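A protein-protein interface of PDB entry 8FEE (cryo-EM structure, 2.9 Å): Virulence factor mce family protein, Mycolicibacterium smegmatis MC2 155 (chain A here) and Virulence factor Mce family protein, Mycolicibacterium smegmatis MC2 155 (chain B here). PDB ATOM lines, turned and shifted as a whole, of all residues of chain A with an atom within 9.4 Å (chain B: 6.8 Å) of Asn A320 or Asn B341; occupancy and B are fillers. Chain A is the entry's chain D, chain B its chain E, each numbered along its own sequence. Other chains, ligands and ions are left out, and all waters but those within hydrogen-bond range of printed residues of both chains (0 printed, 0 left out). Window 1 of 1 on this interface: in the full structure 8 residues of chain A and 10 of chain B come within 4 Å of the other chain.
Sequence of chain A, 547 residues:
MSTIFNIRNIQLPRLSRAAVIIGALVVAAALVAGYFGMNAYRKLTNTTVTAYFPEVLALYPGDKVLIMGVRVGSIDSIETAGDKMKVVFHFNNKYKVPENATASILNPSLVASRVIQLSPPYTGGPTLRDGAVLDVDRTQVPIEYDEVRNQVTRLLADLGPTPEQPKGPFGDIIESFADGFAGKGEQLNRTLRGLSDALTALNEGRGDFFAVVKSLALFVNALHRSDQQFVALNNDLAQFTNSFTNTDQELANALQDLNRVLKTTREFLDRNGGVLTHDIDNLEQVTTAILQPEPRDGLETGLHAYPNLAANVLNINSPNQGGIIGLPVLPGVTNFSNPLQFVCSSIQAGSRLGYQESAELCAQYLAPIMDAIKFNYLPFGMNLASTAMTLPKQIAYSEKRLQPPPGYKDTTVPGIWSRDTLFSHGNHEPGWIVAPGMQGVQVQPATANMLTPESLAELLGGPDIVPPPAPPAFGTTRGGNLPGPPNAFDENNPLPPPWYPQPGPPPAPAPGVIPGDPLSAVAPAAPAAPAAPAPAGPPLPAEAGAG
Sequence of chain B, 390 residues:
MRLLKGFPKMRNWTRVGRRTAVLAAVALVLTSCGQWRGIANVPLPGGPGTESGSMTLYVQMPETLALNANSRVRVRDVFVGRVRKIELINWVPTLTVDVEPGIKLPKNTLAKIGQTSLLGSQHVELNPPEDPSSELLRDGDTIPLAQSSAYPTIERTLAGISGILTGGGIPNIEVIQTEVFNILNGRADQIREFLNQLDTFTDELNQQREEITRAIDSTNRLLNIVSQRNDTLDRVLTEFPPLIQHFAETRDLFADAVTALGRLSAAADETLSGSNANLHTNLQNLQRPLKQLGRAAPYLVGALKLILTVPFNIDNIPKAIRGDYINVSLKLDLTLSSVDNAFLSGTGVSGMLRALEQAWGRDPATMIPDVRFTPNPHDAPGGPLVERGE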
ATOM      1  N   ILE A 316     -20.106   4.422  -7.049  1.00  0.00           N
ATOM      2  CA  ILE A 316     -19.299   4.888  -5.923  1.00  0.00           C
ATOM      3  C   ILE A 316     -17.809   4.797  -6.246  1.00  0.00           C
ATOM      4  O   ILE A 316     -17.020   5.667  -5.857  1.00  0.00           O
ATOM      5  CB  ILE A 316     -19.659   4.095  -4.654  1.00  0.00           C
ATOM      6  CG1 ILE A 316     -21.068   4.457  -4.193  1.00  0.00           C
ATOM      7  CG2 ILE A 316     -18.694   4.394  -3.534  1.00  0.00           C
ATOM      8  CD1 ILE A 316     -21.476   3.793  -2.904  1.00  0.00           C
ATOM      9  N   ASN A 317     -17.407   3.766  -6.982  1.00  0.00           N
ATOM     10  CA  ASN A 317     -15.995   3.509  -7.240  1.00  0.00           C
ATOM     11  C   ASN A 317     -15.380   4.579  -8.136  1.00  0.00           C
ATOM     12  O   ASN A 317     -15.942   4.931  -9.178  1.00  0.00           O
ATOM     13  CB  ASN A 317     -15.832   2.134  -7.881  1.00  0.00           C
ATOM     14  CG  ASN A 317     -16.706   1.087  -7.228  1.00  0.00           C
ATOM     15  OD1 ASN A 317     -16.492   0.714  -6.077  1.00  0.00           O
ATOM     16  ND2 ASN A 317     -17.686   0.590  -7.968  1.00  0.00           N
ATOM     17  N   SER A 318     -14.220   5.086  -7.732  1.00  0.00           N
ATOM     18  CA  SER A 318     -13.502   6.122  -8.477  1.00  0.00           C
ATOM     19  C   SER A 318     -12.175   5.577  -8.986  1.00  0.00           C
ATOM     20  O   SER A 318     -11.283   5.270  -8.172  1.00  0.00           O
ATOM     21  CB  SER A 318     -13.267   7.347  -7.596  1.00  0.00           C
ATOM     22  OG  SER A 318     -12.778   6.965  -6.324  1.00  0.00           O
ATOM     23  N   PRO A 319     -12.001   5.427 -10.303  1.00  0.00           N
ATOM     24  CA  PRO A 319     -10.788   4.770 -10.825  1.00  0.00           C
ATOM     25  C   PRO A 319      -9.481   5.468 -10.484  1.00  0.00           C
ATOM     26  O   PRO A 319      -8.461   4.787 -10.321  1.00  0.00           O
ATOM     27  CB  PRO A 319     -11.029   4.756 -12.340  1.00  0.00           C
ATOM     28  CG  PRO A 319     -12.500   4.883 -12.500  1.00  0.00           C
ATOM     29  CD  PRO A 319     -12.965   5.739 -11.368  1.00  0.00           C
ATOM     30  N   ASN A 320      -9.470   6.801 -10.388  1.00  0.00           N
ATOM     31  CA  ASN A 320      -8.218   7.514 -10.141  1.00  0.00           C
ATOM     32  C   ASN A 320      -7.680   7.243  -8.743  1.00  0.00           C
ATOM     33  O   ASN A 320      -6.472   7.047  -8.565  1.00  0.00           O
ATOM     34  CB  ASN A 320      -8.410   9.014 -10.353  1.00  0.00           C
ATOM     35  CG  ASN A 320      -8.505   9.386 -11.815  1.00  0.00           C
ATOM     36  OD1 ASN A 320      -8.171   8.589 -12.691  1.00  0.00           O
ATOM     37  ND2 ASN A 320      -8.955  10.604 -12.088  1.00  0.00           N
ATOM     38  N   GLN A 321      -8.550   7.244  -7.739  1.00  0.00           N
ATOM     39  CA  GLN A 321      -8.143   7.010  -6.363  1.00  0.00           C
ATOM     40  C   GLN A 321      -8.312   5.560  -5.931  1.00  0.00           C
ATOM     41  O   GLN A 321      -7.780   5.176  -4.885  1.00  0.00           O
ATOM     42  CB  GLN A 321      -8.928   7.919  -5.405  1.00  0.00           C
ATOM     43  CG  GLN A 321      -8.809   9.415  -5.676  1.00  0.00           C
ATOM     44  CD  GLN A 321      -9.722   9.895  -6.787  1.00  0.00           C
ATOM     45  OE1 GLN A 321     -10.541   9.137  -7.303  1.00  0.00           O
ATOM     46  NE2 GLN A 321      -9.582  11.161  -7.162  1.00  0.00           N
ATOM     47  N   GLY A 322      -9.035   4.753  -6.702  1.00  0.00           N
ATOM     48  CA  GLY A 322      -9.268   3.365  -6.359  1.00  0.00           C
ATOM     49  C   GLY A 322     -10.275   3.186  -5.243  1.00  0.00           C
ATOM     50  O   GLY A 322     -10.514   4.110  -4.459  1.00  0.00           O
ATOM     51  N   GLY A 323     -10.870   1.998  -5.157  1.00  0.00           N
ATOM     52  CA  GLY A 323     -11.759   1.700  -4.052  1.00  0.00           C
ATOM     53  C   GLY A 323     -13.034   2.524  -4.105  1.00  0.00           C
ATOM     54  O   GLY A 323     -13.495   2.946  -5.168  1.00  0.00           O
ATOM     55  N   ILE A 325     -15.833   5.478  -1.992  1.00  0.00           N
ATOM     56  CA  ILE A 325     -15.849   6.802  -1.379  1.00  0.00           C
ATOM     57  C   ILE A 325     -17.077   6.894  -0.487  1.00  0.00           C
ATOM     58  O   ILE A 325     -18.168   6.469  -0.877  1.00  0.00           O
ATOM     59  CB  ILE A 325     -15.867   7.928  -2.438  1.00  0.00           C
ATOM     60  CG1 ILE A 325     -14.672   7.821  -3.386  1.00  0.00           C
ATOM     61  CG2 ILE A 325     -15.887   9.296  -1.777  1.00  0.00           C
ATOM     62  CD1 ILE A 325     -14.700   8.833  -4.500  1.00  0.00           C
ATOM     63  N   THR A 387     -13.441  16.652  -6.322  1.00  0.00           N
ATOM     64  CA  THR A 387     -12.171  16.241  -6.897  1.00  0.00           C
ATOM     65  C   THR A 387     -12.390  15.406  -8.159  1.00  0.00           C
ATOM     66  O   THR A 387     -13.490  14.923  -8.441  1.00  0.00           O
ATOM     67  CB  THR A 387     -11.356  15.451  -5.879  1.00  0.00           C
ATOM     68  OG1 THR A 387     -12.139  14.350  -5.407  1.00  0.00           O
ATOM     69  CG2 THR A 387     -10.972  16.336  -4.707  1.00  0.00           C
ATOM     70  N   ALA A 388     -11.313  15.236  -8.920  1.00  0.00           N
ATOM     71  CA  ALA A 388     -11.358  14.524 -10.193  1.00  0.00           C
ATOM     72  C   ALA A 388     -11.408  13.025  -9.925  1.00  0.00           C
ATOM     73  O   ALA A 388     -10.408  12.428  -9.511  1.00  0.00           O
ATOM     74  CB  ALA A 388     -10.154  14.889 -11.053  1.00  0.00           C
ATOM     75  N   MET A 389     -12.571  12.416 -10.155  1.00  0.00           N
ATOM     76  CA  MET A 389     -12.728  10.982  -9.930  1.00  0.00           C
ATOM     77  C   MET A 389     -12.175  10.152 -11.083  1.00  0.00           C
ATOM     78  O   MET A 389     -11.583   9.093 -10.854  1.00  0.00           O
ATOM     79  CB  MET A 389     -14.197  10.638  -9.690  1.00  0.00           C
ATOM     80  CG  MET A 389     -14.809  11.325  -8.488  1.00  0.00           C
ATOM     81  SD  MET A 389     -16.436  10.668  -8.095  1.00  0.00           S
ATOM     82  CE  MET A 389     -16.969  11.829  -6.843  1.00  0.00           C
ATOM     83  N   THR A 390     -12.366  10.597 -12.323  1.00  0.00           N
ATOM     84  CA  THR A 390     -11.968   9.830 -13.497  1.00  0.00           C
ATOM     85  C   THR A 390     -11.154  10.714 -14.436  1.00  0.00           C
ATOM     86  O   THR A 390     -10.917  11.895 -14.167  1.00  0.00           O
ATOM     87  CB  THR A 390     -13.184   9.263 -14.244  1.00  0.00           C
ATOM     88  OG1 THR A 390     -13.849  10.321 -14.944  1.00  0.00           O
ATOM     89  CG2 THR A 390     -14.169   8.608 -13.287  1.00  0.00           C
ATOM     90  N   LEU A 391     -10.736  10.129 -15.551  1.00  0.00           N
ATOM     91  CA  LEU A 391      -9.954  10.784 -16.588  1.00  0.00           C
ATOM     92  C   LEU A 391     -10.607  10.540 -17.937  1.00  0.00           C
ATOM     93  O   LEU A 391     -11.348   9.566 -18.110  1.00  0.00           O
ATOM     94  CB  LEU A 391      -8.508  10.260 -16.613  1.00  0.00           C
ATOM     95  CG  LEU A 391      -7.554  10.633 -15.477  1.00  0.00           C
ATOM     96  CD1 LEU A 391      -6.116  10.466 -15.937  1.00  0.00           C
ATOM     97  CD2 LEU A 391      -7.794  12.053 -14.997  1.00  0.00           C
ATOM     98  N   PRO A 392     -10.368  11.421 -18.915  1.00  0.00           N
ATOM     99  CA  PRO A 392     -10.938  11.198 -20.256  1.00  0.00           C
ATOM    100  C   PRO A 392     -10.483   9.909 -20.916  1.00  0.00           C
ATOM    101  O   PRO A 392     -11.216   9.361 -21.749  1.00  0.00           O
ATOM    102  CB  PRO A 392     -10.462  12.427 -21.043  1.00  0.00           C
ATOM    103  CG  PRO A 392     -10.241  13.472 -20.006  1.00  0.00           C
ATOM    104  CD  PRO A 392      -9.723  12.740 -18.806  1.00  0.00           C
ATOM    105  N   LYS A 393      -9.299   9.408 -20.577  1.00  0.00           N
ATOM    106  CA  LYS A 393      -8.766   8.192 -21.178  1.00  0.00           C
ATOM    107  C   LYS A 393      -9.172   6.930 -20.429  1.00  0.00           C
ATOM    108  O   LYS A 393      -8.736   5.838 -20.806  1.00  0.00           O
ATOM    109  CB  LYS A 393      -7.240   8.269 -21.258  1.00  0.00           C
ATOM    110  CG  LYS A 393      -6.554   8.315 -19.906  1.00  0.00           C
ATOM    111  CD  LYS A 393      -5.049   8.171 -20.045  1.00  0.00           C
ATOM    112  CE  LYS A 393      -4.378   8.101 -18.685  1.00  0.00           C
ATOM    113  NZ  LYS A 393      -2.908   7.906 -18.803  1.00  0.00           N
ATOM    114  N   GLN A 394      -9.984   7.049 -19.379  1.00  0.00           N
ATOM    115  CA  GLN A 394     -10.442   5.896 -18.620  1.00  0.00           C
ATOM    116  C   GLN A 394     -11.909   5.553 -18.838  1.00  0.00           C
ATOM    117  O   GLN A 394     -12.329   4.457 -18.455  1.00  0.00           O
ATOM    118  CB  GLN A 394     -10.198   6.120 -17.120  1.00  0.00           C
ATOM    119  CG  GLN A 394      -8.734   6.122 -16.722  1.00  0.00           C
ATOM    120  CD  GLN A 394      -8.533   6.489 -15.268  1.00  0.00           C
ATOM    121  OE1 GLN A 394      -9.490   6.570 -14.501  1.00  0.00           O
ATOM    122  NE2 GLN A 394      -7.283   6.716 -14.881  1.00  0.00           N
ATOM    123  N   ILE A 395     -12.700   6.444 -19.427  1.00  0.00           N
ATOM    124  CA  ILE A 395     -14.128   6.191 -19.592  1.00  0.00           C
ATOM    125  C   ILE A 395     -14.337   5.241 -20.763  1.00  0.00           C
ATOM    126  O   ILE A 395     -13.808   5.460 -21.859  1.00  0.00           O
ATOM    127  CB  ILE A 395     -14.893   7.505 -19.804  1.00  0.00           C
ATOM    128  CG1 ILE A 395     -14.460   8.545 -18.772  1.00  0.00           C
ATOM    129  CG2 ILE A 395     -16.389   7.263 -19.717  1.00  0.00           C
ATOM    130  CD1 ILE A 395     -14.960   8.265 -17.378  1.00  0.00           C
ATOM    131  N   LEU B 336       2.416  11.555   0.123  1.00  0.00           N
ATOM    132  CA  LEU B 336       2.439  12.519  -0.973  1.00  0.00           C
ATOM    133  C   LEU B 336       1.725  11.977  -2.204  1.00  0.00           C
ATOM    134  O   LEU B 336       0.963  12.699  -2.855  1.00  0.00           O
ATOM    135  CB  LEU B 336       3.879  12.905  -1.314  1.00  0.00           C
ATOM    136  CG  LEU B 336       4.605  13.827  -0.333  1.00  0.00           C
ATOM    137  CD1 LEU B 336       5.953  14.248  -0.895  1.00  0.00           C
ATOM    138  CD2 LEU B 336       3.757  15.044   0.005  1.00  0.00           C
ATOM    139  N   SER B 337       1.963  10.706  -2.542  1.00  0.00           N
ATOM    140  CA  SER B 337       1.318  10.117  -3.713  1.00  0.00           C
ATOM    141  C   SER B 337      -0.187   9.989  -3.514  1.00  0.00           C
ATOM    142  O   SER B 337      -0.963  10.192  -4.456  1.00  0.00           O
ATOM    143  CB  SER B 337       1.933   8.754  -4.020  1.00  0.00           C
ATOM    144  OG  SER B 337       1.716   7.845  -2.956  1.00  0.00           O
ATOM    145  N   SER B 338      -0.616   9.640  -2.298  1.00  0.00           N
ATOM    146  CA  SER B 338      -2.044   9.522  -2.019  1.00  0.00           C
ATOM    147  C   SER B 338      -2.750  10.864  -2.166  1.00  0.00           C
ATOM    148  O   SER B 338      -3.838  10.940  -2.749  1.00  0.00           O
ATOM    149  CB  SER B 338      -2.260   8.953  -0.617  1.00  0.00           C
ATOM    150  OG  SER B 338      -1.792   9.851   0.373  1.00  0.00           O
ATOM    151  N   VAL B 339      -2.146  11.935  -1.647  1.00  0.00           N
ATOM    152  CA  VAL B 339      -2.738  13.263  -1.780  1.00  0.00           C
ATOM    153  C   VAL B 339      -2.685  13.730  -3.232  1.00  0.00           C
ATOM    154  O   VAL B 339      -3.607  14.397  -3.719  1.00  0.00           O
ATOM    155  CB  VAL B 339      -2.034  14.248  -0.828  1.00  0.00           C
ATOM    156  CG1 VAL B 339      -2.444  15.684  -1.118  1.00  0.00           C
ATOM    157  CG2 VAL B 339      -2.346  13.892   0.617  1.00  0.00           C
ATOM    158  N   ASP B 340      -1.617  13.374  -3.948  1.00  0.00           N
ATOM    159  CA  ASP B 340      -1.511  13.716  -5.363  1.00  0.00           C
ATOM    160  C   ASP B 340      -2.621  13.066  -6.180  1.00  0.00           C
ATOM    161  O   ASP B 340      -3.219  13.708  -7.050  1.00  0.00           O
ATOM    162  CB  ASP B 340      -0.141  13.297  -5.896  1.00  0.00           C
ATOM    163  CG  ASP B 340      -0.184  12.862  -7.347  1.00  0.00           C
ATOM    164  OD1 ASP B 340      -0.548  13.687  -8.210  1.00  0.00           O
ATOM    165  OD2 ASP B 340       0.145  11.690  -7.624  1.00  0.00           O
ATOM    166  N   ASN B 341      -2.907  11.790  -5.918  1.00  0.00           N
ATOM    167  CA  ASN B 341      -3.996  11.127  -6.626  1.00  0.00           C
ATOM    168  C   ASN B 341      -5.358  11.619  -6.158  1.00  0.00           C
ATOM    169  O   ASN B 341      -6.307  11.657  -6.951  1.00  0.00           O
ATOM    170  CB  ASN B 341      -3.892   9.612  -6.462  1.00  0.00           C
ATOM    171  CG  ASN B 341      -3.083   8.963  -7.568  1.00  0.00           C
ATOM    172  OD1 ASN B 341      -2.749   9.603  -8.565  1.00  0.00           O
ATOM    173  ND2 ASN B 341      -2.767   7.686  -7.400  1.00  0.00           N
ATOM    174  N   ALA B 342      -5.478  12.000  -4.886  1.00  0.00           N
ATOM    175  CA  ALA B 342      -6.777  12.396  -4.350  1.00  0.00           C
ATOM    176  C   ALA B 342      -7.195  13.778  -4.837  1.00  0.00           C
ATOM    177  O   ALA B 342      -8.373  14.002  -5.137  1.00  0.00           O
ATOM    178  CB  ALA B 342      -6.747  12.358  -2.824  1.00  0.00           C
ATOM    179  N   PHE B 343      -6.254  14.718  -4.918  1.00  0.00           N
ATOM    180  CA  PHE B 343      -6.572  16.103  -5.243  1.00  0.00           C
ATOM    181  C   PHE B 343      -6.062  16.523  -6.615  1.00  0.00           C
ATOM    182  O   PHE B 343      -6.844  16.983  -7.452  1.00  0.00           O
ATOM    183  CB  PHE B 343      -6.007  17.034  -4.161  1.00  0.00           C
ATOM    184  CG  PHE B 343      -6.794  17.028  -2.883  1.00  0.00           C
ATOM    185  CD1 PHE B 343      -8.084  17.534  -2.847  1.00  0.00           C
ATOM    186  CD2 PHE B 343      -6.245  16.528  -1.716  1.00  0.00           C
ATOM    187  CE1 PHE B 343      -8.811  17.533  -1.671  1.00  0.00           C
ATOM    188  CE2 PHE B 343      -6.966  16.525  -0.536  1.00  0.00           C
ATOM    189  CZ  PHE B 343      -8.251  17.028  -0.515  1.00  0.00           C
ATOM    190  N   LEU B 344      -4.764  16.368  -6.880  1.00  0.00           N
ATOM    191  CA  LEU B 344      -4.120  17.002  -8.024  1.00  0.00           C
ATOM    192  C   LEU B 344      -4.069  16.106  -9.255  1.00  0.00           C
ATOM    193  O   LEU B 344      -3.129  16.210 -10.055  1.00  0.00           O
ATOM    194  CB  LEU B 344      -2.716  17.466  -7.637  1.00  0.00           C
ATOM    195  CG  LEU B 344      -2.659  18.311  -6.363  1.00  0.00           C
ATOM    196  CD1 LEU B 344      -1.239  18.737  -6.068  1.00  0.00           C
ATOM    197  CD2 LEU B 344      -3.566  19.524  -6.482  1.00  0.00           C
ATOM    198  N   SER B 345      -5.048  15.223  -9.426  1.00  0.00           N
ATOM    199  CA  SER B 345      -5.177  14.437 -10.646  1.00  0.00           C
ATOM    200  C   SER B 345      -6.010  15.208 -11.661  1.00  0.00           C
ATOM    201  O   SER B 345      -7.050  15.776 -11.316  1.00  0.00           O
ATOM    202  CB  SER B 345      -5.820  13.083 -10.355  1.00  0.00           C
ATOM    203  OG  SER B 345      -5.070  12.356  -9.401  1.00  0.00           O
ATOM    204  N   GLY B 346      -5.543  15.234 -12.906  1.00  0.00           N
ATOM    205  CA  GLY B 346      -6.240  15.949 -13.955  1.00  0.00           C
ATOM    206  C   GLY B 346      -5.969  17.433 -14.022  1.00  0.00           C
ATOM    207  O   GLY B 346      -6.637  18.132 -14.790  1.00  0.00           O
ATOM    208  N   SER B 350       0.100  17.679 -11.479  1.00  0.00           N
ATOM    209  CA  SER B 350       0.049  16.246 -11.201  1.00  0.00           C
ATOM    210  C   SER B 350       1.386  15.735 -10.673  1.00  0.00           C
ATOM    211  O   SER B 350       1.434  15.000  -9.679  1.00  0.00           O
ATOM    212  CB  SER B 350      -0.360  15.487 -12.463  1.00  0.00           C
ATOM    213  OG  SER B 350      -0.361  14.089 -12.241  1.00  0.00           O
ATOM    214  N   LEU B 353       4.420  16.760  -6.658  1.00  0.00           N
ATOM    215  CA  LEU B 353       4.850  16.075  -5.448  1.00  0.00           C
ATOM    216  C   LEU B 353       5.027  14.572  -5.607  1.00  0.00           C
ATOM    217  O   LEU B 353       5.757  13.974  -4.809  1.00  0.00           O
ATOM    218  CB  LEU B 353       3.871  16.341  -4.288  1.00  0.00           C
ATOM    219  CG  LEU B 353       2.411  15.870  -4.258  1.00  0.00           C
ATOM    220  CD1 LEU B 353       1.796  16.258  -2.927  1.00  0.00           C
ATOM    221  CD2 LEU B 353       1.572  16.447  -5.380  1.00  0.00           C
ATOM    222  N   ARG B 354       4.404  13.950  -6.610  1.00  0.00           N
ATOM    223  CA  ARG B 354       4.687  12.546  -6.898  1.00  0.00           C
ATOM    224  C   ARG B 354       6.163  12.342  -7.214  1.00  0.00           C
ATOM    225  O   ARG B 354       6.816  11.459  -6.646  1.00  0.00           O
ATOM    226  CB  ARG B 354       3.816  12.060  -8.055  1.00  0.00           C
ATOM    227  CG  ARG B 354       4.347  10.816  -8.749  1.00  0.00           C
ATOM    228  CD  ARG B 354       3.787   9.552  -8.127  1.00  0.00           C
ATOM    229  NE  ARG B 354       2.369   9.683  -7.817  1.00  0.00           N
ATOM    230  CZ  ARG B 354       1.577   8.671  -7.491  1.00  0.00           C
ATOM    231  NH1 ARG B 354       2.026   7.427  -7.457  1.00  0.00           N
ATOM    232  NH2 ARG B 354       0.303   8.913  -7.200  1.00  0.00           N
ATOM    233  N   ILE B 368       1.153   3.884  -5.196  1.00  0.00           N
ATOM    234  CA  ILE B 368      -0.070   3.715  -5.988  1.00  0.00           C
ATOM    235  C   ILE B 368       0.193   4.200  -7.411  1.00  0.00           C
ATOM    236  O   ILE B 368       0.783   5.284  -7.593  1.00  0.00           O
ATOM    237  CB  ILE B 368      -1.241   4.476  -5.329  1.00  0.00           C
ATOM    238  CG1 ILE B 368      -2.489   4.482  -6.213  1.00  0.00           C
ATOM    239  CG2 ILE B 368      -0.831   5.890  -4.936  1.00  0.00           C
ATOM    240  CD1 ILE B 368      -3.709   5.044  -5.523  1.00  0.00           C
ATOM    241  N   PRO B 369      -0.170   3.429  -8.442  1.00  0.00           N
ATOM    242  CA  PRO B 369       0.385   3.663  -9.784  1.00  0.00           C
ATOM    243  C   PRO B 369       0.080   5.052 -10.327  1.00  0.00           C
ATOM    244  O   PRO B 369      -0.990   5.615 -10.091  1.00  0.00           O
ATOM    245  CB  PRO B 369      -0.273   2.570 -10.631  1.00  0.00           C
ATOM    246  CG  PRO B 369      -0.582   1.493  -9.653  1.00  0.00           C
ATOM    247  CD  PRO B 369      -0.989   2.206  -8.402  1.00  0.00           C
ATOM    248  N   ASP B 370       1.048   5.600 -11.059  1.00  0.00           N
ATOM    249  CA  ASP B 370       0.914   6.923 -11.660  1.00  0.00           C
ATOM    250  C   ASP B 370      -0.031   6.837 -12.850  1.00  0.00           C
ATOM    251  O   ASP B 370       0.329   6.290 -13.898  1.00  0.00           O
ATOM    252  CB  ASP B 370       2.283   7.445 -12.084  1.00  0.00           C
ATOM    253  CG  ASP B 370       3.291   7.423 -10.952  1.00  0.00           C
ATOM    254  OD1 ASP B 370       2.948   6.930  -9.857  1.00  0.00           O
ATOM    255  OD2 ASP B 370       4.427   7.898 -11.154  1.00  0.00           O
ATOM    256  N   VAL B 371      -1.239   7.389 -12.692  1.00  0.00           N
ATOM    257  CA  VAL B 371      -2.308   7.215 -13.670  1.00  0.00           C
ATOM    258  C   VAL B 371      -1.956   7.779 -15.039  1.00  0.00           C
ATOM    259  O   VAL B 371      -2.600   7.425 -16.032  1.00  0.00           O
ATOM    260  CB  VAL B 371      -3.613   7.852 -13.149  1.00  0.00           C
ATOM    261  CG1 VAL B 371      -4.191   7.027 -12.012  1.00  0.00           C
ATOM    262  CG2 VAL B 371      -3.365   9.284 -12.703  1.00  0.00           C
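Hydrophobic or aromatic side chains of chain A that line the printed part of chain B: Ala A388. Printed residues of chain B that touch a printed residue of chain A: Asn B341, Ala B342, Phe B343, Ser B345 and Val B371. Along chain B the printed residues that touch a printed residue of chain A span positions 341 to 371. Among the printed residues, no Asp or Glu carboxylate lies within 4 Å of a Lys or Arg side-chain nitrogen of the other chain.
The backbone carbonyl oxygen (O) of Asn B341 lies within hydrogen-bond range of the side-chain amide nitrogen (NE2) of Gln A321. NZ of Lys A393 sits at hydrogen-bond distance from O of Val B371, 2.8 Å away.
Of chain B, only Asn B341 (3.9 Å) comes within 4 Å of Asn A320. Asn B341 touches just these residues of chain A: Asn A320 (3.9 Å) and Gln A321 (3.3 Å). Of chain A, only Gln A321 and Thr A387 come within 4 Å of Ala B342. Printed residues of chain A within 4 Å of Ser B345: Ala A388. Printed residues of chain B within 4 Å of Ala A388: Ser B345 (3.2 Å). The nearest residue of chain B that does not touch Asn A320 is Val B371 (4.1 Å). The nearest residue of chain A that does not touch Asn B341 is Ala A388 (4.9 Å). The nearest printed residue of chain B that does not touch Ala A388 is Asn B341 (4.9 Å).
The backbone NH (N) of Asn A320 sits at hydrogen-bond distance from the backbone carbonyl oxygen (O) of Met A389 (3.2 Å). ND2 of Asn B341 lies close to NH2 of Arg B354 (3.3 Å). OG of Ser B345 sits at hydrogen-bond distance from O of Asp B340, 3.3 Å away. The side-chain hydroxyl (OG) of Ser A318 lies within hydrogen-bond range of the side-chain amide oxygen (OE1) of Gln A321 (3.3 Å). O of Asn B341 lies within hydrogen-bond range of OG of Ser B345. The backbone carbonyl oxygen (O) of Ala A388 lies within hydrogen-bond range of the side-chain amide nitrogen (NE2) of Gln A321 (2.8 Å).
Asn A320 touches Asn B341 (O to ND2, 3.9 Å). Gln A321 touches Ala B342. CB of Thr A387 touches O of Ala B342, 3.4 Å away. CG2 of Thr A387 touches CD1 of Phe B343, at 3.6 Å. CB of Ala A388 touches O of Ser B345, at 3.2 Å.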
